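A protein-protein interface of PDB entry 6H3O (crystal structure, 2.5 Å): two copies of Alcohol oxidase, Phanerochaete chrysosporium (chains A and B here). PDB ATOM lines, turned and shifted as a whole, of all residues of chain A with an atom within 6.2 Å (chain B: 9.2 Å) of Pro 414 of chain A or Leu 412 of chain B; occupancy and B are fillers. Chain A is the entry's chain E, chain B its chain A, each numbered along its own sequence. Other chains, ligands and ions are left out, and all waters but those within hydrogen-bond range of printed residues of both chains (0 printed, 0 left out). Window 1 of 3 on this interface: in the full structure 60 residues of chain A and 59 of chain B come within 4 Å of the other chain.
The guanidinium group (NH2) of Arg 321 of chain A lies within hydrogen-bond range of the backbone carbonyl oxygen (O) of Thr 411 of chain B, at 2.8 Å.
CD of Pro 415 of chain B touches O of His 410 of chain A (3.3 Å). His 410 of chain A touches Tyr 509 of chain B (O to CE2, 3.9 Å). Pro 414 of chain B touches Leu 413 of chain A (CA to O, 3.4 Å). CG of Pro 414 of chain A touches C of Leu 412 of chain B, 3.9 Å away. Pro 414 of chain A touches Leu 413 of chain B (CA to O, 3.4 Å). Pro 415 of chain A touches His 410 of chain B. Ser 484 of chain A touches Ser 484 of chain B. Ile 500 of chain A touches Thr 411 of chain B. CG2 of Ile 500 of chain A touches CD2 of Leu 412 of chain B, 3.6 Å away. CG of Trp 522 of chain A touches CD2 of His 485 of chain B, 3.2 Å away.
Of the 17 printed residues of chain A, 12 touch a printed residue of chain B. Hydrophobic or aromatic side chains of chain A within 4 Å of the printed part of chain B: His 410, Pro 414, Pro 415, Ile 500, Trp 522 and His 523. Of the 18 printed residues of chain B, 9 touch a printed residue of chain A. Printed residues of chain B that touch a printed residue of chain A: His 410, Thr 411, Leu 412, Leu 413, Pro 414, Pro 415, Ser 484, His 485 and Tyr 509. Hydrophobic or aromatic side chains of chain B that line the printed part of chain A: Leu 412, Pro 414, Pro 415, His 485 and Tyr 509. Among the printed residues, 19 pairs touch across the chains. Among the printed residues, no Asp or Glu carboxylate lies within 4 Å of a Lys or Arg side-chain nitrogen of the other chain.
His 410 of chain A touches Pro 415 of chain B, and with the chains exchanged Pro 415 of chain A touches His 410 of chain B. Leu 412 of chain A touches Pro 414 of chain B, and with the chains exchanged Pro 414 of chain A touches Leu 412 of chain B. Leu 413 of chain A touches Pro 414 of chain B, and with the chains exchanged Pro 414 of chain A touches Leu 413 of chain B. Leu 413 of chain A touches Pro 415 of chain B, and with the chains exchanged Pro 415 of chain A touches Leu 413 of chain B. Positions printed for both chains: 321, 334, 410, 412, 413, 414, 415, 416, 418, 482, 484 and 485.
OD1 of Asp 409 of chain B sits close to N of Thr 411 of chain B (3.1 Å). O of Pro 415 of chain A lies within hydrogen-bond range of NH2 of Arg 321 of chain A (2.9 Å). NH2 of Arg 334 of chain A sits at hydrogen-bond distance from O of Pro 414 of chain A (2.6 Å). The guanidinium group (NH1) of Arg 334 of chain A lies within hydrogen-bond range of the backbone carbonyl oxygen (O) of Gly 416 of chain A. The backbone carbonyl oxygen (O) of Pro 415 of chain A sits at hydrogen-bond distance from the side-chain hydroxyl (OH) of Tyr 418 of chain A (3.4 Å). The side-chain carboxylate (OD2) of Asp 499 of chain A is in hydrogen-bond range of the side-chain hydroxyl (OG1) of Thr 483 of chain A (2.5 Å).
Pro 414 of chain A touches just these residues of chain B: Thr 411, Leu 412 and Leu 413. Of chain A, only Pro 414, Asp 499, Ile 500 and His 523 come within 4 Å of Leu 412 of chain B. Of the printed residues of chain B, Pro 415 of chain A touches His 410, Thr 411 and Leu 413. Of the printed residues of chain A, Pro 415 of chain B touches His 410 (3.3 Å) and Leu 413 (3.3 Å). Printed residues of chain A within 4 Å of His 410 of chain B: Pro 415. Of the printed residues of chain B, Leu 412 of chain A touches Pro 414 (3.9 Å). Of the printed residues of chain A, His 485 of chain B touches Trp 522 (3.2 Å). The nearest residue of chain A that does not touch Leu 412 of chain B is Arg 321 of chain A (4.6 Å). The nearest printed residue of chain B that does not touch His 410 of chain A is Pro 414 of chain B (4.8 Å).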
ATOM      1  N   ARG A 321     -13.964   6.717  12.096  1.00  0.00           N
ATOM      2  CA  ARG A 321     -14.296   7.819  12.984  1.00  0.00           C
ATOM      3  C   ARG A 321     -13.402   9.005  12.620  1.00  0.00           C
ATOM      4  O   ARG A 321     -12.216   8.797  12.298  1.00  0.00           O
ATOM      5  CB  ARG A 321     -14.093   7.403  14.442  1.00  0.00           C
ATOM      6  CG  ARG A 321     -14.977   6.247  14.896  1.00  0.00           C
ATOM      7  CD  ARG A 321     -14.741   5.933  16.360  1.00  0.00           C
ATOM      8  NE  ARG A 321     -15.941   5.879  17.192  1.00  0.00           N
ATOM      9  CZ  ARG A 321     -16.711   6.927  17.488  1.00  0.00           C
ATOM     10  NH1 ARG A 321     -16.686   8.017  16.738  1.00  0.00           N
ATOM     11  NH2 ARG A 321     -17.512   6.880  18.538  1.00  0.00           N
ATOM     12  N   ARG A 334     -28.886  12.326  11.995  1.00  0.00           N
ATOM     13  CA  ARG A 334     -29.390  11.896  13.306  1.00  0.00           C
ATOM     14  C   ARG A 334     -30.707  12.633  13.611  1.00  0.00           C
ATOM     15  O   ARG A 334     -31.487  12.202  14.468  1.00  0.00           O
ATOM     16  CB  ARG A 334     -28.350  12.139  14.408  1.00  0.00           C
ATOM     17  CG  ARG A 334     -27.249  11.093  14.481  1.00  0.00           C
ATOM     18  CD  ARG A 334     -26.189  11.463  15.505  1.00  0.00           C
ATOM     19  NE  ARG A 334     -25.238  10.382  15.699  1.00  0.00           N
ATOM     20  CZ  ARG A 334     -23.922  10.466  15.532  1.00  0.00           C
ATOM     21  NH1 ARG A 334     -23.350  11.605  15.178  1.00  0.00           N
ATOM     22  NH2 ARG A 334     -23.173   9.403  15.756  1.00  0.00           N
ATOM     23  N   HIS A 410     -27.666   4.944  12.112  1.00  0.00           N
ATOM     24  CA  HIS A 410     -26.962   5.652  13.238  1.00  0.00           C
ATOM     25  C   HIS A 410     -27.431   5.122  14.597  1.00  0.00           C
ATOM     26  O   HIS A 410     -26.916   5.502  15.655  1.00  0.00           O
ATOM     27  CB  HIS A 410     -27.186   7.171  13.184  1.00  0.00           C
ATOM     28  CG  HIS A 410     -26.367   7.877  12.157  1.00  0.00           C
ATOM     29  ND1 HIS A 410     -26.627   7.775  10.803  1.00  0.00           N
ATOM     30  CD2 HIS A 410     -25.299   8.697  12.277  1.00  0.00           C
ATOM     31  CE1 HIS A 410     -25.745   8.486  10.134  1.00  0.00           C
ATOM     32  NE2 HIS A 410     -24.926   9.073  11.015  1.00  0.00           N
ATOM     33  N   LEU A 412     -27.189   2.074  15.265  1.00  0.00           N
ATOM     34  CA  LEU A 412     -26.115   1.094  15.576  1.00  0.00           C
ATOM     35  C   LEU A 412     -24.740   1.783  15.535  1.00  0.00           C
ATOM     36  O   LEU A 412     -23.712   1.110  15.590  1.00  0.00           O
ATOM     37  CB  LEU A 412     -26.140  -0.049  14.549  1.00  0.00           C
ATOM     38  CG  LEU A 412     -27.046  -1.254  14.828  1.00  0.00           C
ATOM     39  CD1 LEU A 412     -26.613  -2.000  16.078  1.00  0.00           C
ATOM     40  CD2 LEU A 412     -28.517  -0.850  14.912  1.00  0.00           C
ATOM     41  N   LEU A 413     -24.698   3.113  15.412  1.00  0.00           N
ATOM     42  CA  LEU A 413     -23.428   3.830  15.418  1.00  0.00           C
ATOM     43  C   LEU A 413     -23.288   4.586  16.730  1.00  0.00           C
ATOM     44  O   LEU A 413     -24.233   5.226  17.173  1.00  0.00           O
ATOM     45  CB  LEU A 413     -23.358   4.822  14.251  1.00  0.00           C
ATOM     46  CG  LEU A 413     -23.311   4.230  12.843  1.00  0.00           C
ATOM     47  CD1 LEU A 413     -23.388   5.351  11.818  1.00  0.00           C
ATOM     48  CD2 LEU A 413     -22.056   3.399  12.621  1.00  0.00           C
ATOM     49  N   PRO A 414     -22.092   4.582  17.359  1.00  0.00           N
ATOM     50  CA  PRO A 414     -21.834   5.444  18.503  1.00  0.00           C
ATOM     51  C   PRO A 414     -22.162   6.893  18.176  1.00  0.00           C
ATOM     52  O   PRO A 414     -22.541   7.222  17.053  1.00  0.00           O
ATOM     53  CB  PRO A 414     -20.326   5.303  18.734  1.00  0.00           C
ATOM     54  CG  PRO A 414     -19.977   3.963  18.169  1.00  0.00           C
ATOM     55  CD  PRO A 414     -20.925   3.759  17.007  1.00  0.00           C
ATOM     56  N   PRO A 415     -21.983   7.816  19.140  1.00  0.00           N
ATOM     57  CA  PRO A 415     -21.972   9.242  18.826  1.00  0.00           C
ATOM     58  C   PRO A 415     -20.635   9.651  18.182  1.00  0.00           C
ATOM     59  O   PRO A 415     -19.669   8.836  18.113  1.00  0.00           O
ATOM     60  CB  PRO A 415     -22.145   9.883  20.206  1.00  0.00           C
ATOM     61  CG  PRO A 415     -21.432   8.915  21.129  1.00  0.00           C
ATOM     62  CD  PRO A 415     -21.735   7.542  20.564  1.00  0.00           C
ATOM     63  N   GLY A 416     -20.578  10.913  17.738  1.00  0.00           N
ATOM     64  CA  GLY A 416     -19.425  11.461  17.047  1.00  0.00           C
ATOM     65  C   GLY A 416     -19.567  11.325  15.541  1.00  0.00           C
ATOM     66  O   GLY A 416     -20.626  10.906  15.027  1.00  0.00           O
ATOM     67  N   TYR A 418     -18.274  10.534  11.485  1.00  0.00           N
ATOM     68  CA  TYR A 418     -17.758   9.476  10.634  1.00  0.00           C
ATOM     69  C   TYR A 418     -17.589   9.970   9.194  1.00  0.00           C
ATOM     70  O   TYR A 418     -18.254  10.894   8.746  1.00  0.00           O
ATOM     71  CB  TYR A 418     -18.696   8.268  10.643  1.00  0.00           C
ATOM     72  CG  TYR A 418     -19.008   7.737  12.019  1.00  0.00           C
ATOM     73  CD1 TYR A 418     -18.164   6.827  12.640  1.00  0.00           C
ATOM     74  CD2 TYR A 418     -20.132   8.156  12.710  1.00  0.00           C
ATOM     75  CE1 TYR A 418     -18.429   6.345  13.912  1.00  0.00           C
ATOM     76  CE2 TYR A 418     -20.408   7.686  13.986  1.00  0.00           C
ATOM     77  CZ  TYR A 418     -19.551   6.781  14.588  1.00  0.00           C
ATOM     78  OH  TYR A 418     -19.807   6.306  15.837  1.00  0.00           O
ATOM     79  N   LEU A 482     -14.071   2.193  13.003  1.00  0.00           N
ATOM     80  CA  LEU A 482     -15.186   1.776  13.882  1.00  0.00           C
ATOM     81  C   LEU A 482     -15.131   0.248  14.025  1.00  0.00           C
ATOM     82  O   LEU A 482     -15.567  -0.499  13.118  1.00  0.00           O
ATOM     83  CB  LEU A 482     -16.536   2.247  13.321  1.00  0.00           C
ATOM     84  CG  LEU A 482     -17.749   1.960  14.213  1.00  0.00           C
ATOM     85  CD1 LEU A 482     -17.692   2.739  15.524  1.00  0.00           C
ATOM     86  CD2 LEU A 482     -19.049   2.260  13.481  1.00  0.00           C
ATOM     87  N   THR A 483     -14.575  -0.199  15.160  1.00  0.00           N
ATOM     88  CA  THR A 483     -14.265  -1.609  15.425  1.00  0.00           C
ATOM     89  C   THR A 483     -15.465  -2.488  15.062  1.00  0.00           C
ATOM     90  O   THR A 483     -15.321  -3.449  14.297  1.00  0.00           O
ATOM     91  CB  THR A 483     -13.868  -1.806  16.891  1.00  0.00           C
ATOM     92  OG1 THR A 483     -12.969  -0.756  17.248  1.00  0.00           O
ATOM     93  CG2 THR A 483     -13.245  -3.159  17.159  1.00  0.00           C
ATOM     94  N   SER A 484     -16.644  -2.106  15.581  1.00  0.00           N
ATOM     95  CA  SER A 484     -17.873  -2.914  15.542  1.00  0.00           C
ATOM     96  C   SER A 484     -18.287  -3.246  14.105  1.00  0.00           C
ATOM     97  O   SER A 484     -18.773  -4.337  13.877  1.00  0.00           O
ATOM     98  CB  SER A 484     -19.013  -2.254  16.304  1.00  0.00           C
ATOM     99  OG  SER A 484     -19.400  -1.012  15.728  1.00  0.00           O
ATOM    100  N   HIS A 485     -18.080  -2.313  13.162  1.00  0.00           N
ATOM    101  CA  HIS A 485     -18.606  -2.400  11.776  1.00  0.00           C
ATOM    102  C   HIS A 485     -17.525  -2.892  10.797  1.00  0.00           C
ATOM    103  O   HIS A 485     -17.681  -2.761   9.560  1.00  0.00           O
ATOM    104  CB  HIS A 485     -19.160  -1.034  11.329  1.00  0.00           C
ATOM    105  CG  HIS A 485     -20.529  -0.718  11.829  1.00  0.00           C
ATOM    106  ND1 HIS A 485     -20.877  -0.856  13.149  1.00  0.00           N
ATOM    107  CD2 HIS A 485     -21.619  -0.227  11.195  1.00  0.00           C
ATOM    108  CE1 HIS A 485     -22.137  -0.491  13.304  1.00  0.00           C
ATOM    109  NE2 HIS A 485     -22.621  -0.103  12.116  1.00  0.00           N
ATOM    110  N   ASP A 499      -9.653   2.167  17.319  1.00  0.00           N
ATOM    111  CA  ASP A 499     -10.902   2.933  17.348  1.00  0.00           C
ATOM    112  C   ASP A 499     -10.585   4.360  17.820  1.00  0.00           C
ATOM    113  O   ASP A 499      -9.448   4.808  17.673  1.00  0.00           O
ATOM    114  CB  ASP A 499     -11.941   2.199  18.203  1.00  0.00           C
ATOM    115  CG  ASP A 499     -13.394   2.458  17.833  1.00  0.00           C
ATOM    116  OD1 ASP A 499     -13.829   3.630  17.934  1.00  0.00           O
ATOM    117  OD2 ASP A 499     -14.085   1.482  17.474  1.00  0.00           O
ATOM    118  N   ILE A 500     -11.584   5.047  18.397  1.00  0.00           N
ATOM    119  CA  ILE A 500     -11.497   6.478  18.756  1.00  0.00           C
ATOM    120  C   ILE A 500     -10.417   6.673  19.824  1.00  0.00           C
ATOM    121  O   ILE A 500     -10.281   5.857  20.738  1.00  0.00           O
ATOM    122  CB  ILE A 500     -12.859   7.037  19.236  1.00  0.00           C
ATOM    123  CG1 ILE A 500     -12.891   8.566  19.190  1.00  0.00           C
ATOM    124  CG2 ILE A 500     -13.225   6.510  20.618  1.00  0.00           C
ATOM    125  CD1 ILE A 500     -14.271   9.164  19.375  1.00  0.00           C
ATOM    126  N   TRP A 522     -13.754  -3.127  24.712  1.00  0.00           N
ATOM    127  CA  TRP A 522     -14.547  -3.241  23.506  1.00  0.00           C
ATOM    128  C   TRP A 522     -13.795  -2.653  22.307  1.00  0.00           C
ATOM    129  O   TRP A 522     -14.087  -2.997  21.168  1.00  0.00           O
ATOM    130  CB  TRP A 522     -15.893  -2.545  23.731  1.00  0.00           C
ATOM    131  CG  TRP A 522     -16.568  -3.017  24.981  1.00  0.00           C
ATOM    132  CD1 TRP A 522     -16.811  -2.303  26.116  1.00  0.00           C
ATOM    133  CD2 TRP A 522     -17.049  -4.349  25.231  1.00  0.00           C
ATOM    134  NE1 TRP A 522     -17.438  -3.091  27.044  1.00  0.00           N
ATOM    135  CE2 TRP A 522     -17.597  -4.352  26.531  1.00  0.00           C
ATOM    136  CE3 TRP A 522     -17.090  -5.531  24.480  1.00  0.00           C
ATOM    137  CZ2 TRP A 522     -18.170  -5.495  27.093  1.00  0.00           C
ATOM    138  CZ3 TRP A 522     -17.655  -6.657  25.037  1.00  0.00           C
ATOM    139  CH2 TRP A 522     -18.184  -6.640  26.327  1.00  0.00           C
ATOM    140  N   HIS A 523     -12.837  -1.765  22.588  1.00  0.00           N
ATOM    141  CA  HIS A 523     -12.069  -1.083  21.583  1.00  0.00           C
ATOM    142  C   HIS A 523     -10.634  -0.896  22.082  1.00  0.00           C
ATOM    143  O   HIS A 523     -10.415  -0.606  23.250  1.00  0.00           O
ATOM    144  CB  HIS A 523     -12.730   0.257  21.232  1.00  0.00           C
ATOM    145  CG  HIS A 523     -12.531   1.341  22.241  1.00  0.00           C
ATOM    146  ND1 HIS A 523     -13.198   1.369  23.451  1.00  0.00           N
ATOM    147  CD2 HIS A 523     -11.761   2.451  22.216  1.00  0.00           C
ATOM    148  CE1 HIS A 523     -12.834   2.437  24.131  1.00  0.00           C
ATOM    149  NE2 HIS A 523     -11.956   3.119  23.393  1.00  0.00           N
ATOM    150  N   ILE B 319     -24.207  -6.495  27.672  1.00  0.00           N
ATOM    151  CA  ILE B 319     -25.015  -5.289  27.524  1.00  0.00           C
ATOM    152  C   ILE B 319     -26.196  -5.578  26.599  1.00  0.00           C
ATOM    153  O   ILE B 319     -26.036  -6.182  25.519  1.00  0.00           O
ATOM    154  CB  ILE B 319     -24.184  -4.105  27.003  1.00  0.00           C
ATOM    155  CG1 ILE B 319     -22.929  -3.900  27.854  1.00  0.00           C
ATOM    156  CG2 ILE B 319     -25.052  -2.853  26.929  1.00  0.00           C
ATOM    157  CD1 ILE B 319     -21.994  -2.837  27.335  1.00  0.00           C
ATOM    158  N   ARG B 321     -30.082  -3.960  25.070  1.00  0.00           N
ATOM    159  CA  ARG B 321     -30.860  -2.793  24.705  1.00  0.00           C
ATOM    160  C   ARG B 321     -32.277  -2.968  25.257  1.00  0.00           C
ATOM    161  O   ARG B 321     -32.801  -4.069  25.225  1.00  0.00           O
ATOM    162  CB  ARG B 321     -30.842  -2.633  23.185  1.00  0.00           C
ATOM    163  CG  ARG B 321     -29.476  -2.251  22.634  1.00  0.00           C
ATOM    164  CD  ARG B 321     -29.473  -2.193  21.121  1.00  0.00           C
ATOM    165  NE  ARG B 321     -29.007  -0.931  20.551  1.00  0.00           N
ATOM    166  CZ  ARG B 321     -29.624   0.241  20.684  1.00  0.00           C
ATOM    167  NH1 ARG B 321     -30.477   0.444  21.678  1.00  0.00           N
ATOM    168  NH2 ARG B 321     -29.374   1.215  19.824  1.00  0.00           N
ATOM    169  N   ARG B 334     -24.209  10.079  29.861  1.00  0.00           N
ATOM    170  CA  ARG B 334     -23.834  10.811  28.621  1.00  0.00           C
ATOM    171  C   ARG B 334     -23.510  12.276  28.952  1.00  0.00           C
ATOM    172  O   ARG B 334     -22.739  12.936  28.247  1.00  0.00           O
ATOM    173  CB  ARG B 334     -24.945  10.757  27.568  1.00  0.00           C
ATOM    174  CG  ARG B 334     -25.094   9.403  26.888  1.00  0.00           C
ATOM    175  CD  ARG B 334     -26.294   9.292  25.971  1.00  0.00           C
ATOM    176  NE  ARG B 334     -26.226   8.097  25.137  1.00  0.00           N
ATOM    177  CZ  ARG B 334     -27.083   7.079  25.163  1.00  0.00           C
ATOM    178  NH1 ARG B 334     -28.208   7.154  25.854  1.00  0.00           N
ATOM    179  NH2 ARG B 334     -26.812   5.985  24.475  1.00  0.00           N
ATOM    180  N   ALA B 406     -26.063   1.157  30.897  1.00  0.00           N
ATOM    181  CA  ALA B 406     -24.831   0.623  30.324  1.00  0.00           C
ATOM    182  C   ALA B 406     -23.626   1.037  31.184  1.00  0.00           C
ATOM    183  O   ALA B 406     -23.223   2.202  31.180  1.00  0.00           O
ATOM    184  CB  ALA B 406     -24.673   1.121  28.913  1.00  0.00           C
ATOM    185  N   ALA B 408     -20.280   1.036  30.713  1.00  0.00           N
ATOM    186  CA  ALA B 408     -19.482   0.983  29.481  1.00  0.00           C
ATOM    187  C   ALA B 408     -19.324   2.404  28.924  1.00  0.00           C
ATOM    188  O   ALA B 408     -20.154   3.279  29.179  1.00  0.00           O
ATOM    189  CB  ALA B 408     -20.127   0.073  28.454  1.00  0.00           C
ATOM    190  N   ASP B 409     -18.258   2.597  28.146  1.00  0.00           N
ATOM    191  CA  ASP B 409     -17.902   3.872  27.572  1.00  0.00           C
ATOM    192  C   ASP B 409     -18.921   4.259  26.493  1.00  0.00           C
ATOM    193  O   ASP B 409     -18.825   3.792  25.364  1.00  0.00           O
ATOM    194  CB  ASP B 409     -16.488   3.816  26.999  1.00  0.00           C
ATOM    195  CG  ASP B 409     -16.000   5.160  26.506  1.00  0.00           C
ATOM    196  OD1 ASP B 409     -16.849   6.062  26.347  1.00  0.00           O
ATOM    197  OD2 ASP B 409     -14.775   5.295  26.282  1.00  0.00           O
ATOM    198  N   HIS B 410     -19.845   5.162  26.852  1.00  0.00           N
ATOM    199  CA  HIS B 410     -20.995   5.569  26.021  1.00  0.00           C
ATOM    200  C   HIS B 410     -20.559   6.157  24.672  1.00  0.00           C
ATOM    201  O   HIS B 410     -21.355   6.201  23.726  1.00  0.00           O
ATOM    202  CB  HIS B 410     -21.887   6.551  26.790  1.00  0.00           C
ATOM    203  CG  HIS B 410     -22.828   5.871  27.721  1.00  0.00           C
ATOM    204  ND1 HIS B 410     -22.415   5.365  28.933  1.00  0.00           N
ATOM    205  CD2 HIS B 410     -24.146   5.590  27.614  1.00  0.00           C
ATOM    206  CE1 HIS B 410     -23.448   4.818  29.545  1.00  0.00           C
ATOM    207  NE2 HIS B 410     -24.523   4.939  28.759  1.00  0.00           N
ATOM    208  N   THR B 411     -19.303   6.604  24.600  1.00  0.00           N
ATOM    209  CA  THR B 411     -18.656   7.080  23.385  1.00  0.00           C
ATOM    210  C   THR B 411     -18.484   5.932  22.368  1.00  0.00           C
ATOM    211  O   THR B 411     -18.132   6.161  21.207  1.00  0.00           O
ATOM    212  CB  THR B 411     -17.354   7.790  23.789  1.00  0.00           C
ATOM    213  OG1 THR B 411     -17.512   9.188  23.516  1.00  0.00           O
ATOM    214  CG2 THR B 411     -16.119   7.226  23.120  1.00  0.00           C
ATOM    215  N   LEU B 412     -18.722   4.690  22.803  1.00  0.00           N
ATOM    216  CA  LEU B 412     -18.558   3.511  21.972  1.00  0.00           C
ATOM    217  C   LEU B 412     -19.874   2.721  21.883  1.00  0.00           C
ATOM    218  O   LEU B 412     -19.874   1.607  21.391  1.00  0.00           O
ATOM    219  CB  LEU B 412     -17.435   2.663  22.586  1.00  0.00           C
ATOM    220  CG  LEU B 412     -16.185   2.470  21.733  1.00  0.00           C
ATOM    221  CD1 LEU B 412     -16.516   1.674  20.482  1.00  0.00           C
ATOM    222  CD2 LEU B 412     -15.545   3.804  21.374  1.00  0.00           C
ATOM    223  N   LEU B 413     -20.987   3.320  22.331  1.00  0.00           N
ATOM    224  CA  LEU B 413     -22.305   2.671  22.377  1.00  0.00           C
ATOM    225  C   LEU B 413     -23.270   3.431  21.478  1.00  0.00           C
ATOM    226  O   LEU B 413     -23.282   4.655  21.518  1.00  0.00           O
ATOM    227  CB  LEU B 413     -22.822   2.694  23.819  1.00  0.00           C
ATOM    228  CG  LEU B 413     -22.085   1.801  24.813  1.00  0.00           C
ATOM    229  CD1 LEU B 413     -22.497   2.137  26.236  1.00  0.00           C
ATOM    230  CD2 LEU B 413     -22.354   0.332  24.521  1.00  0.00           C
ATOM    231  N   PRO B 414     -24.120   2.761  20.665  1.00  0.00           N
ATOM    232  CA  PRO B 414     -25.146   3.460  19.896  1.00  0.00           C
ATOM    233  C   PRO B 414     -25.986   4.283  20.855  1.00  0.00           C
ATOM    234  O   PRO B 414     -25.801   4.162  22.063  1.00  0.00           O
ATOM    235  CB  PRO B 414     -26.014   2.375  19.248  1.00  0.00           C
ATOM    236  CG  PRO B 414     -25.193   1.084  19.360  1.00  0.00           C
ATOM    237  CD  PRO B 414     -24.150   1.306  20.443  1.00  0.00           C
ATOM    238  N   PRO B 415     -26.905   5.143  20.359  1.00  0.00           N
ATOM    239  CA  PRO B 415     -27.886   5.803  21.217  1.00  0.00           C
ATOM    240  C   PRO B 415     -28.925   4.793  21.718  1.00  0.00           C
ATOM    241  O   PRO B 415     -28.881   3.607  21.320  1.00  0.00           O
ATOM    242  CB  PRO B 415     -28.539   6.838  20.294  1.00  0.00           C
ATOM    243  CG  PRO B 415     -28.407   6.214  18.926  1.00  0.00           C
ATOM    244  CD  PRO B 415     -27.051   5.535  18.952  1.00  0.00           C
ATOM    245  N   GLY B 416     -29.857   5.282  22.551  1.00  0.00           N
ATOM    246  CA  GLY B 416     -30.866   4.465  23.219  1.00  0.00           C
ATOM    247  C   GLY B 416     -30.487   4.177  24.664  1.00  0.00           C
ATOM    248  O   GLY B 416     -29.387   4.551  25.117  1.00  0.00           O
ATOM    249  N   TYR B 418     -30.017   1.285  27.815  1.00  0.00           N
ATOM    250  CA  TYR B 418     -29.456  -0.070  28.007  1.00  0.00           C
ATOM    251  C   TYR B 418     -29.611  -0.568  29.450  1.00  0.00           C
ATOM    252  O   TYR B 418     -29.829   0.207  30.379  1.00  0.00           O
ATOM    253  CB  TYR B 418     -27.951  -0.094  27.732  1.00  0.00           C
ATOM    254  CG  TYR B 418     -27.564   0.377  26.358  1.00  0.00           C
ATOM    255  CD1 TYR B 418     -27.651  -0.470  25.268  1.00  0.00           C
ATOM    256  CD2 TYR B 418     -27.114   1.669  26.149  1.00  0.00           C
ATOM    257  CE1 TYR B 418     -27.283  -0.049  24.003  1.00  0.00           C
ATOM    258  CE2 TYR B 418     -26.757   2.111  24.888  1.00  0.00           C
ATOM    259  CZ  TYR B 418     -26.844   1.248  23.812  1.00  0.00           C
ATOM    260  OH  TYR B 418     -26.487   1.660  22.563  1.00  0.00           O
ATOM    261  N   LEU B 482     -26.827  -5.921  22.284  1.00  0.00           N
ATOM    262  CA  LEU B 482     -25.950  -5.025  21.562  1.00  0.00           C
ATOM    263  C   LEU B 482     -24.895  -5.867  20.838  1.00  0.00           C
ATOM    264  O   LEU B 482     -23.856  -6.170  21.407  1.00  0.00           O
ATOM    265  CB  LEU B 482     -25.314  -4.012  22.523  1.00  0.00           C
ATOM    266  CG  LEU B 482     -24.448  -2.949  21.845  1.00  0.00           C
ATOM    267  CD1 LEU B 482     -25.233  -2.194  20.788  1.00  0.00           C
ATOM    268  CD2 LEU B 482     -23.865  -1.983  22.854  1.00  0.00           C
ATOM    269  N   SER B 484     -22.560  -5.517  18.907  1.00  0.00           N
ATOM    270  CA  SER B 484     -21.189  -5.014  18.914  1.00  0.00           C
ATOM    271  C   SER B 484     -20.400  -5.523  20.131  1.00  0.00           C
ATOM    272  O   SER B 484     -19.247  -5.902  19.970  1.00  0.00           O
ATOM    273  CB  SER B 484     -21.162  -3.502  18.829  1.00  0.00           C
ATOM    274  OG  SER B 484     -21.673  -2.897  20.007  1.00  0.00           O
ATOM    275  N   HIS B 485     -21.022  -5.533  21.319  1.00  0.00           N
ATOM    276  CA  HIS B 485     -20.360  -5.870  22.607  1.00  0.00           C
ATOM    277  C   HIS B 485     -20.676  -7.316  23.045  1.00  0.00           C
ATOM    278  O   HIS B 485     -20.761  -7.597  24.248  1.00  0.00           O
ATOM    279  CB  HIS B 485     -20.784  -4.875  23.705  1.00  0.00           C
ATOM    280  CG  HIS B 485     -20.230  -3.493  23.569  1.00  0.00           C
ATOM    281  ND1 HIS B 485     -20.257  -2.787  22.379  1.00  0.00           N
ATOM    282  CD2 HIS B 485     -19.674  -2.667  24.486  1.00  0.00           C
ATOM    283  CE1 HIS B 485     -19.712  -1.601  22.565  1.00  0.00           C
ATOM    284  NE2 HIS B 485     -19.348  -1.499  23.859  1.00  0.00           N
ATOM    285  N   TYR B 509     -34.533   8.340  17.093  1.00  0.00           N
ATOM    286  CA  TYR B 509     -34.328   9.422  16.122  1.00  0.00           C
ATOM    287  C   TYR B 509     -35.577   9.556  15.246  1.00  0.00           C
ATOM    288  O   TYR B 509     -35.563   9.117  14.102  1.00  0.00           O
ATOM    289  CB  TYR B 509     -33.089   9.146  15.253  1.00  0.00           C
ATOM    290  CG  TYR B 509     -31.746   9.191  15.948  1.00  0.00           C
ATOM    291  CD1 TYR B 509     -31.459  10.143  16.916  1.00  0.00           C
ATOM    292  CD2 TYR B 509     -30.734   8.305  15.602  1.00  0.00           C
ATOM    293  CE1 TYR B 509     -30.219  10.203  17.533  1.00  0.00           C
ATOM    294  CE2 TYR B 509     -29.488   8.351  16.209  1.00  0.00           C
ATOM    295  CZ  TYR B 509     -29.231   9.305  17.177  1.00  0.00           C
ATOM    296  OH  TYR B 509     -28.016   9.368  17.789  1.00  0.00           O
